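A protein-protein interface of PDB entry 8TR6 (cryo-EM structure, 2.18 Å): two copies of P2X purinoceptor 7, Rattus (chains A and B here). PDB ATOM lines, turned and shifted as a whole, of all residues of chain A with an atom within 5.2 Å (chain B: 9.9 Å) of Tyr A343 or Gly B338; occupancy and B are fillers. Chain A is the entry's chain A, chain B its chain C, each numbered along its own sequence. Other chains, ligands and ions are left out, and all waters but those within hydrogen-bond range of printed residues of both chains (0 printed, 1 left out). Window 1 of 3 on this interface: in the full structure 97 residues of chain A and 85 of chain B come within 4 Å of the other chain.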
ATOM      1  N   VAL A  37       9.484  16.279   1.050  1.00  0.00           N
ATOM      2  CA  VAL A  37       9.762  15.778   2.394  1.00  0.00           C
ATOM      3  C   VAL A  37      10.195  14.319   2.333  1.00  0.00           C
ATOM      4  O   VAL A  37      11.173  13.918   2.975  1.00  0.00           O
ATOM      5  CB  VAL A  37       8.530  15.963   3.300  1.00  0.00           C
ATOM      6  CG1 VAL A  37       8.674  15.151   4.581  1.00  0.00           C
ATOM      7  CG2 VAL A  37       8.323  17.432   3.617  1.00  0.00           C
ATOM      8  N   GLY A 338       9.859   7.829  13.018  1.00  0.00           N
ATOM      9  CA  GLY A 338       9.013   8.588  13.920  1.00  0.00           C
ATOM     10  C   GLY A 338       9.443  10.037  14.031  1.00  0.00           C
ATOM     11  O   GLY A 338       8.607  10.940  14.106  1.00  0.00           O
ATOM     12  N   SER A 339      10.756  10.277  14.046  1.00  0.00           N
ATOM     13  CA  SER A 339      11.258  11.644  14.111  1.00  0.00           C
ATOM     14  C   SER A 339      10.879  12.428  12.862  1.00  0.00           C
ATOM     15  O   SER A 339      10.584  13.624  12.937  1.00  0.00           O
ATOM     16  CB  SER A 339      12.775  11.635  14.298  1.00  0.00           C
ATOM     17  OG  SER A 339      13.442  11.374  13.077  1.00  0.00           O
ATOM     18  N   THR A 340      10.884  11.773  11.705  1.00  0.00           N
ATOM     19  CA  THR A 340      10.597  12.454  10.448  1.00  0.00           C
ATOM     20  C   THR A 340       9.114  12.487  10.088  1.00  0.00           C
ATOM     21  O   THR A 340       8.741  13.199   9.151  1.00  0.00           O
ATOM     22  CB  THR A 340      11.372  11.790   9.306  1.00  0.00           C
ATOM     23  OG1 THR A 340      11.252  10.367   9.403  1.00  0.00           O
ATOM     24  CG2 THR A 340      12.839  12.177   9.366  1.00  0.00           C
ATOM     25  N   LEU A 341       8.264  11.747  10.802  1.00  0.00           N
ATOM     26  CA  LEU A 341       6.852  11.685  10.437  1.00  0.00           C
ATOM     27  C   LEU A 341       6.190  13.058  10.497  1.00  0.00           C
ATOM     28  O   LEU A 341       5.397  13.409   9.617  1.00  0.00           O
ATOM     29  CB  LEU A 341       6.117  10.706  11.353  1.00  0.00           C
ATOM     30  CG  LEU A 341       6.104   9.229  10.950  1.00  0.00           C
ATOM     31  CD1 LEU A 341       5.406   8.396  12.013  1.00  0.00           C
ATOM     32  CD2 LEU A 341       5.461   9.027   9.591  1.00  0.00           C
ATOM     33  N   SER A 342       6.497  13.846  11.529  1.00  0.00           N
ATOM     34  CA  SER A 342       5.846  15.140  11.690  1.00  0.00           C
ATOM     35  C   SER A 342       6.124  16.083  10.528  1.00  0.00           C
ATOM     36  O   SER A 342       5.355  17.027  10.316  1.00  0.00           O
ATOM     37  CB  SER A 342       6.288  15.792  12.998  1.00  0.00           C
ATOM     38  OG  SER A 342       5.539  15.299  14.090  1.00  0.00           O
ATOM     39  N   TYR A 343       7.201  15.859   9.774  1.00  0.00           N
ATOM     40  CA  TYR A 343       7.519  16.739   8.658  1.00  0.00           C
ATOM     41  C   TYR A 343       6.530  16.601   7.511  1.00  0.00           C
ATOM     42  O   TYR A 343       6.465  17.490   6.656  1.00  0.00           O
ATOM     43  CB  TYR A 343       8.938  16.463   8.158  1.00  0.00           C
ATOM     44  CG  TYR A 343      10.007  17.184   8.942  1.00  0.00           C
ATOM     45  CD1 TYR A 343      10.009  18.566   9.038  1.00  0.00           C
ATOM     46  CD2 TYR A 343      11.014  16.483   9.586  1.00  0.00           C
ATOM     47  CE1 TYR A 343      10.978  19.230   9.750  1.00  0.00           C
ATOM     48  CE2 TYR A 343      11.990  17.140  10.302  1.00  0.00           C
ATOM     49  CZ  TYR A 343      11.968  18.512  10.380  1.00  0.00           C
ATOM     50  OH  TYR A 343      12.939  19.173  11.093  1.00  0.00           O
ATOM     51  N   PHE A 344       5.760  15.513   7.470  1.00  0.00           N
ATOM     52  CA  PHE A 344       4.772  15.336   6.416  1.00  0.00           C
ATOM     53  C   PHE A 344       3.551  16.225   6.604  1.00  0.00           C
ATOM     54  O   PHE A 344       2.712  16.295   5.701  1.00  0.00           O
ATOM     55  CB  PHE A 344       4.356  13.868   6.339  1.00  0.00           C
ATOM     56  CG  PHE A 344       5.392  12.989   5.708  1.00  0.00           C
ATOM     57  CD1 PHE A 344       5.597  13.016   4.341  1.00  0.00           C
ATOM     58  CD2 PHE A 344       6.174  12.151   6.480  1.00  0.00           C
ATOM     59  CE1 PHE A 344       6.555  12.215   3.756  1.00  0.00           C
ATOM     60  CE2 PHE A 344       7.132  11.349   5.900  1.00  0.00           C
ATOM     61  CZ  PHE A 344       7.323  11.382   4.537  1.00  0.00           C
ATOM     62  N   GLY A 345       3.431  16.897   7.746  1.00  0.00           N
ATOM     63  CA  GLY A 345       2.411  17.898   7.955  1.00  0.00           C
ATOM     64  C   GLY A 345       2.757  19.257   7.398  1.00  0.00           C
ATOM     65  O   GLY A 345       2.002  20.214   7.591  1.00  0.00           O
ATOM     66  N   LEU A 346       3.900  19.364   6.717  1.00  0.00           N
ATOM     67  CA  LEU A 346       4.317  20.638   6.146  1.00  0.00           C
ATOM     68  C   LEU A 346       3.328  21.122   5.095  1.00  0.00           C
ATOM     69  O   LEU A 346       3.017  22.315   5.030  1.00  0.00           O
ATOM     70  CB  LEU A 346       5.717  20.500   5.544  1.00  0.00           C
ATOM     71  CG  LEU A 346       6.244  21.634   4.661  1.00  0.00           C
ATOM     72  CD1 LEU A 346       6.638  22.831   5.506  1.00  0.00           C
ATOM     73  CD2 LEU A 346       7.419  21.152   3.830  1.00  0.00           C
ATOM     74  N   ALA A 347       2.834  20.213   4.252  1.00  0.00           N
ATOM     75  CA  ALA A 347       1.868  20.604   3.233  1.00  0.00           C
ATOM     76  C   ALA A 347       0.605  21.163   3.872  1.00  0.00           C
ATOM     77  O   ALA A 347       0.087  22.205   3.452  1.00  0.00           O
ATOM     78  CB  ALA A 347       1.537  19.409   2.341  1.00  0.00           C
ATOM     79  N   VAL B  41      12.737  23.026  24.046  1.00  0.00           N
ATOM     80  CA  VAL B  41      13.338  22.416  22.863  1.00  0.00           C
ATOM     81  C   VAL B  41      14.603  23.168  22.469  1.00  0.00           C
ATOM     82  O   VAL B  41      15.641  22.563  22.178  1.00  0.00           O
ATOM     83  CB  VAL B  41      12.315  22.370  21.712  1.00  0.00           C
ATOM     84  CG1 VAL B  41      12.996  22.111  20.376  1.00  0.00           C
ATOM     85  CG2 VAL B  41      11.269  21.308  21.988  1.00  0.00           C
ATOM     86  N   LEU B  45      18.437  21.886  22.538  1.00  0.00           N
ATOM     87  CA  LEU B  45      19.203  21.930  21.299  1.00  0.00           C
ATOM     88  C   LEU B  45      20.553  22.608  21.502  1.00  0.00           C
ATOM     89  O   LEU B  45      21.580  22.121  21.015  1.00  0.00           O
ATOM     90  CB  LEU B  45      18.397  22.659  20.224  1.00  0.00           C
ATOM     91  CG  LEU B  45      19.062  22.858  18.864  1.00  0.00           C
ATOM     92  CD1 LEU B  45      19.504  21.526  18.285  1.00  0.00           C
ATOM     93  CD2 LEU B  45      18.124  23.578  17.916  1.00  0.00           C
ATOM     94  N   LEU B  50      22.647  19.419  20.040  1.00  0.00           N
ATOM     95  CA  LEU B  50      21.998  18.372  19.262  1.00  0.00           C
ATOM     96  C   LEU B  50      21.957  18.685  17.774  1.00  0.00           C
ATOM     97  O   LEU B  50      21.650  17.791  16.979  1.00  0.00           O
ATOM     98  CB  LEU B  50      20.586  18.134  19.799  1.00  0.00           C
ATOM     99  CG  LEU B  50      20.550  17.667  21.257  1.00  0.00           C
ATOM    100  CD1 LEU B  50      19.124  17.485  21.743  1.00  0.00           C
ATOM    101  CD2 LEU B  50      21.338  16.380  21.431  1.00  0.00           C
ATOM    102  N   ILE B 330      23.281  19.447   9.235  1.00  0.00           N
ATOM    103  CA  ILE B 330      21.884  19.764   8.950  1.00  0.00           C
ATOM    104  C   ILE B 330      20.992  18.563   9.232  1.00  0.00           C
ATOM    105  O   ILE B 330      19.863  18.712   9.712  1.00  0.00           O
ATOM    106  CB  ILE B 330      21.733  20.259   7.498  1.00  0.00           C
ATOM    107  CG1 ILE B 330      20.312  20.772   7.243  1.00  0.00           C
ATOM    108  CG2 ILE B 330      22.057  19.153   6.517  1.00  0.00           C
ATOM    109  CD1 ILE B 330      19.920  21.965   8.089  1.00  0.00           C
ATOM    110  N   ILE B 331      21.474  17.355   8.935  1.00  0.00           N
ATOM    111  CA  ILE B 331      20.655  16.165   9.144  1.00  0.00           C
ATOM    112  C   ILE B 331      20.335  15.984  10.622  1.00  0.00           C
ATOM    113  O   ILE B 331      19.202  15.650  10.987  1.00  0.00           O
ATOM    114  CB  ILE B 331      21.350  14.926   8.552  1.00  0.00           C
ATOM    115  CG1 ILE B 331      21.305  14.981   7.024  1.00  0.00           C
ATOM    116  CG2 ILE B 331      20.689  13.649   9.054  1.00  0.00           C
ATOM    117  CD1 ILE B 331      22.150  13.932   6.338  1.00  0.00           C
ATOM    118  N   GLN B 332      21.325  16.183  11.496  1.00  0.00           N
ATOM    119  CA  GLN B 332      21.079  16.040  12.928  1.00  0.00           C
ATOM    120  C   GLN B 332      20.055  17.057  13.415  1.00  0.00           C
ATOM    121  O   GLN B 332      19.151  16.720  14.191  1.00  0.00           O
ATOM    122  CB  GLN B 332      22.391  16.185  13.702  1.00  0.00           C
ATOM    123  CG  GLN B 332      23.366  15.042  13.487  1.00  0.00           C
ATOM    124  CD  GLN B 332      22.875  13.742  14.084  1.00  0.00           C
ATOM    125  OE1 GLN B 332      22.499  12.819  13.364  1.00  0.00           O
ATOM    126  NE2 GLN B 332      22.877  13.663  15.407  1.00  0.00           N
ATOM    127  N   LEU B 333      20.179  18.309  12.970  1.00  0.00           N
ATOM    128  CA  LEU B 333      19.220  19.332  13.361  1.00  0.00           C
ATOM    129  C   LEU B 333      17.821  18.991  12.866  1.00  0.00           C
ATOM    130  O   LEU B 333      16.838  19.157  13.595  1.00  0.00           O
ATOM    131  CB  LEU B 333      19.664  20.693  12.824  1.00  0.00           C
ATOM    132  CG  LEU B 333      18.694  21.860  13.014  1.00  0.00           C
ATOM    133  CD1 LEU B 333      18.483  22.149  14.488  1.00  0.00           C
ATOM    134  CD2 LEU B 333      19.196  23.091  12.291  1.00  0.00           C
ATOM    135  N   VAL B 334      17.713  18.519  11.622  1.00  0.00           N
ATOM    136  CA  VAL B 334      16.413  18.160  11.066  1.00  0.00           C
ATOM    137  C   VAL B 334      15.796  17.018  11.859  1.00  0.00           C
ATOM    138  O   VAL B 334      14.599  17.034  12.171  1.00  0.00           O
ATOM    139  CB  VAL B 334      16.558  17.805   9.572  1.00  0.00           C
ATOM    140  CG1 VAL B 334      15.287  17.165   9.041  1.00  0.00           C
ATOM    141  CG2 VAL B 334      16.910  19.040   8.765  1.00  0.00           C
ATOM    142  N   VAL B 335      16.600  16.010  12.200  1.00  0.00           N
ATOM    143  CA  VAL B 335      16.094  14.879  12.971  1.00  0.00           C
ATOM    144  C   VAL B 335      15.613  15.339  14.342  1.00  0.00           C
ATOM    145  O   VAL B 335      14.543  14.930  14.807  1.00  0.00           O
ATOM    146  CB  VAL B 335      17.173  13.785  13.079  1.00  0.00           C
ATOM    147  CG1 VAL B 335      16.838  12.798  14.183  1.00  0.00           C
ATOM    148  CG2 VAL B 335      17.329  13.066  11.751  1.00  0.00           C
ATOM    149  N   TYR B 336      16.391  16.195  15.011  1.00  0.00           N
ATOM    150  CA  TYR B 336      15.981  16.675  16.328  1.00  0.00           C
ATOM    151  C   TYR B 336      14.699  17.495  16.247  1.00  0.00           C
ATOM    152  O   TYR B 336      13.795  17.340  17.081  1.00  0.00           O
ATOM    153  CB  TYR B 336      17.093  17.505  16.962  1.00  0.00           C
ATOM    154  CG  TYR B 336      16.656  18.192  18.231  1.00  0.00           C
ATOM    155  CD1 TYR B 336      16.540  17.485  19.415  1.00  0.00           C
ATOM    156  CD2 TYR B 336      16.339  19.541  18.242  1.00  0.00           C
ATOM    157  CE1 TYR B 336      16.131  18.098  20.573  1.00  0.00           C
ATOM    158  CE2 TYR B 336      15.930  20.164  19.397  1.00  0.00           C
ATOM    159  CZ  TYR B 336      15.829  19.439  20.562  1.00  0.00           C
ATOM    160  OH  TYR B 336      15.422  20.052  21.721  1.00  0.00           O
ATOM    161  N   ILE B 337      14.604  18.383  15.256  1.00  0.00           N
ATOM    162  CA  ILE B 337      13.408  19.204  15.107  1.00  0.00           C
ATOM    163  C   ILE B 337      12.198  18.323  14.836  1.00  0.00           C
ATOM    164  O   ILE B 337      11.118  18.543  15.393  1.00  0.00           O
ATOM    165  CB  ILE B 337      13.612  20.253  13.997  1.00  0.00           C
ATOM    166  CG1 ILE B 337      14.556  21.354  14.482  1.00  0.00           C
ATOM    167  CG2 ILE B 337      12.277  20.853  13.569  1.00  0.00           C
ATOM    168  CD1 ILE B 337      15.110  22.217  13.376  1.00  0.00           C
ATOM    169  N   GLY B 338      12.356  17.318  13.975  1.00  0.00           N
ATOM    170  CA  GLY B 338      11.260  16.401  13.721  1.00  0.00           C
ATOM    171  C   GLY B 338      10.849  15.638  14.963  1.00  0.00           C
ATOM    172  O   GLY B 338       9.662  15.400  15.195  1.00  0.00           O
ATOM    173  N   SER B 339      11.828  15.240  15.779  1.00  0.00           N
ATOM    174  CA  SER B 339      11.520  14.534  17.016  1.00  0.00           C
ATOM    175  C   SER B 339      10.744  15.425  17.978  1.00  0.00           C
ATOM    176  O   SER B 339       9.856  14.952  18.694  1.00  0.00           O
ATOM    177  CB  SER B 339      12.809  14.035  17.668  1.00  0.00           C
ATOM    178  OG  SER B 339      13.478  15.082  18.350  1.00  0.00           O
ATOM    179  N   THR B 340      11.068  16.713  18.012  1.00  0.00           N
ATOM    180  CA  THR B 340      10.426  17.631  18.946  1.00  0.00           C
ATOM    181  C   THR B 340       9.147  18.267  18.407  1.00  0.00           C
ATOM    182  O   THR B 340       8.424  18.905  19.178  1.00  0.00           O
ATOM    183  CB  THR B 340      11.404  18.740  19.344  1.00  0.00           C
ATOM    184  OG1 THR B 340      12.069  19.240  18.178  1.00  0.00           O
ATOM    185  CG2 THR B 340      12.435  18.210  20.324  1.00  0.00           C
ATOM    186  N   LEU B 341       8.847  18.107  17.117  1.00  0.00           N
ATOM    187  CA  LEU B 341       7.678  18.769  16.542  1.00  0.00           C
ATOM    188  C   LEU B 341       6.386  18.322  17.217  1.00  0.00           C
ATOM    189  O   LEU B 341       5.504  19.144  17.487  1.00  0.00           O
ATOM    190  CB  LEU B 341       7.609  18.499  15.040  1.00  0.00           C
ATOM    191  CG  LEU B 341       8.380  19.442  14.112  1.00  0.00           C
ATOM    192  CD1 LEU B 341       8.267  18.975  12.670  1.00  0.00           C
ATOM    193  CD2 LEU B 341       7.908  20.876  14.257  1.00  0.00           C
ATOM    194  N   SER B 342       6.250  17.023  17.491  1.00  0.00           N
ATOM    195  CA  SER B 342       5.011  16.514  18.066  1.00  0.00           C
ATOM    196  C   SER B 342       4.708  17.120  19.430  1.00  0.00           C
ATOM    197  O   SER B 342       3.547  17.107  19.853  1.00  0.00           O
ATOM    198  CB  SER B 342       5.071  14.993  18.181  1.00  0.00           C
ATOM    199  OG  SER B 342       4.734  14.377  16.954  1.00  0.00           O
ATOM    200  N   TYR B 343       5.716  17.642  20.129  1.00  0.00           N
ATOM    201  CA  TYR B 343       5.481  18.222  21.444  1.00  0.00           C
ATOM    202  C   TYR B 343       4.689  19.519  21.373  1.00  0.00           C
ATOM    203  O   TYR B 343       4.133  19.947  22.390  1.00  0.00           O
ATOM    204  CB  TYR B 343       6.812  18.464  22.158  1.00  0.00           C
ATOM    205  CG  TYR B 343       7.349  17.245  22.868  1.00  0.00           C
ATOM    206  CD1 TYR B 343       6.611  16.616  23.857  1.00  0.00           C
ATOM    207  CD2 TYR B 343       8.592  16.723  22.547  1.00  0.00           C
ATOM    208  CE1 TYR B 343       7.092  15.505  24.506  1.00  0.00           C
ATOM    209  CE2 TYR B 343       9.084  15.612  23.193  1.00  0.00           C
ATOM    210  CZ  TYR B 343       8.330  15.007  24.172  1.00  0.00           C
ATOM    211  OH  TYR B 343       8.814  13.896  24.820  1.00  0.00           O
ATOM    212  N   PHE B 344       4.622  20.153  20.202  1.00  0.00           N
ATOM    213  CA  PHE B 344       3.854  21.382  20.060  1.00  0.00           C
ATOM    214  C   PHE B 344       2.353  21.133  20.041  1.00  0.00           C
ATOM    215  O   PHE B 344       1.583  22.097  20.090  1.00  0.00           O
ATOM    216  CB  PHE B 344       4.288  22.119  18.795  1.00  0.00           C
ATOM    217  CG  PHE B 344       5.616  22.800  18.930  1.00  0.00           C
ATOM    218  CD1 PHE B 344       5.737  23.964  19.666  1.00  0.00           C
ATOM    219  CD2 PHE B 344       6.747  22.268  18.340  1.00  0.00           C
ATOM    220  CE1 PHE B 344       6.958  24.589  19.800  1.00  0.00           C
ATOM    221  CE2 PHE B 344       7.969  22.888  18.471  1.00  0.00           C
ATOM    222  CZ  PHE B 344       8.075  24.050  19.202  1.00  0.00           C
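O of Ser A339 sits at hydrogen-bond distance from N of Ser B339.
The backbone NH (N) of Gly B338 sits at hydrogen-bond distance from the side-chain hydroxyl (OH) of Tyr A343, at 3.5 Å.
OH of Tyr A343 lies within hydrogen-bond range of O of Val B334 (2.9 Å).
The side-chain hydroxyl of Ser B342 lies within hydrogen-bond range of the side-chain hydroxyl of Ser A342, 3.1 Å away.
The backbone carbonyl oxygen of Gly B338 lies close to the backbone carbonyl oxygen of Ser A339, at 3.0 Å.
O of Tyr B336 lies within hydrogen-bond range of OG of Ser B339.
O of Ile B337 is in hydrogen-bond range of OG1 of Thr B340 (3.0 Å).
Val B335 touches Ser A339.
CB of Leu B341 touches CB of Ser A342, at 3.6 Å.
Ile B337 touches Tyr A343.
Tyr A343 touches Leu B341.
Thr A340 touches none of the printed residues of chain B.
Ser A342 touches two residues of chain B.
Printed residues of chain B within 4 Å of Tyr A343: Val B334 (2.9 Å), Ile B337 (3.1 Å), Gly B338 (3.5 Å) and Leu B341 (3.99 Å).
No residue of chain B comes within 4 Å of Gly A345.
Printed residues of chain A within 4 Å of Val B334: Tyr A343.
Of chain A, only Ser A339 and Tyr A343 come within 4 Å of Gly B338.
Of the printed residues of chain A, Leu B341 touches Ser A342 and Tyr A343.
Of the printed residues of chain A, Ser B342 touches Ser A342 (3.1 Å).
The nearest residue of chain A that does not touch Gly B338 is Ser A342 (4.05 Å).
The nearest printed residue of chain A that does not touch Ser B342 is Gly A338 (5.9 Å).
Of the 11 printed residues of chain A, 3 touch a printed residue of chain B.
Printed residues of chain A that touch a printed residue of chain B: Ser A339, Ser A342 and Tyr A343.
Hydrophobic or aromatic side chains of chain A within 4 Å of the printed part of chain B: Tyr A343.
Hydrophobic or aromatic side chains of chain B within 4 Å of the printed part of chain A: Val B334, Val B335, Ile B337 and Leu B341.
Among the printed residues, 9 pairs touch across the chains.
Ser A339 touches Gly B338, but with the chains exchanged Gly A338 does not touch Ser B339 (5.5 Å).
Ser B339 touches its own counterpart, Ser A339.
Ser A342 touches Leu B341, but with the chains exchanged Leu A341 does not touch Ser B342 (6.7 Å).
Tyr A343 touches Gly B338, but with the chains exchanged Gly A338 does not touch Tyr B343 (9.5 Å).
7 positions are printed for both chains.
Of the 9 pairs that touch across the chains among the printed residues, 2 have their exchanged pair printed and touching as well.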
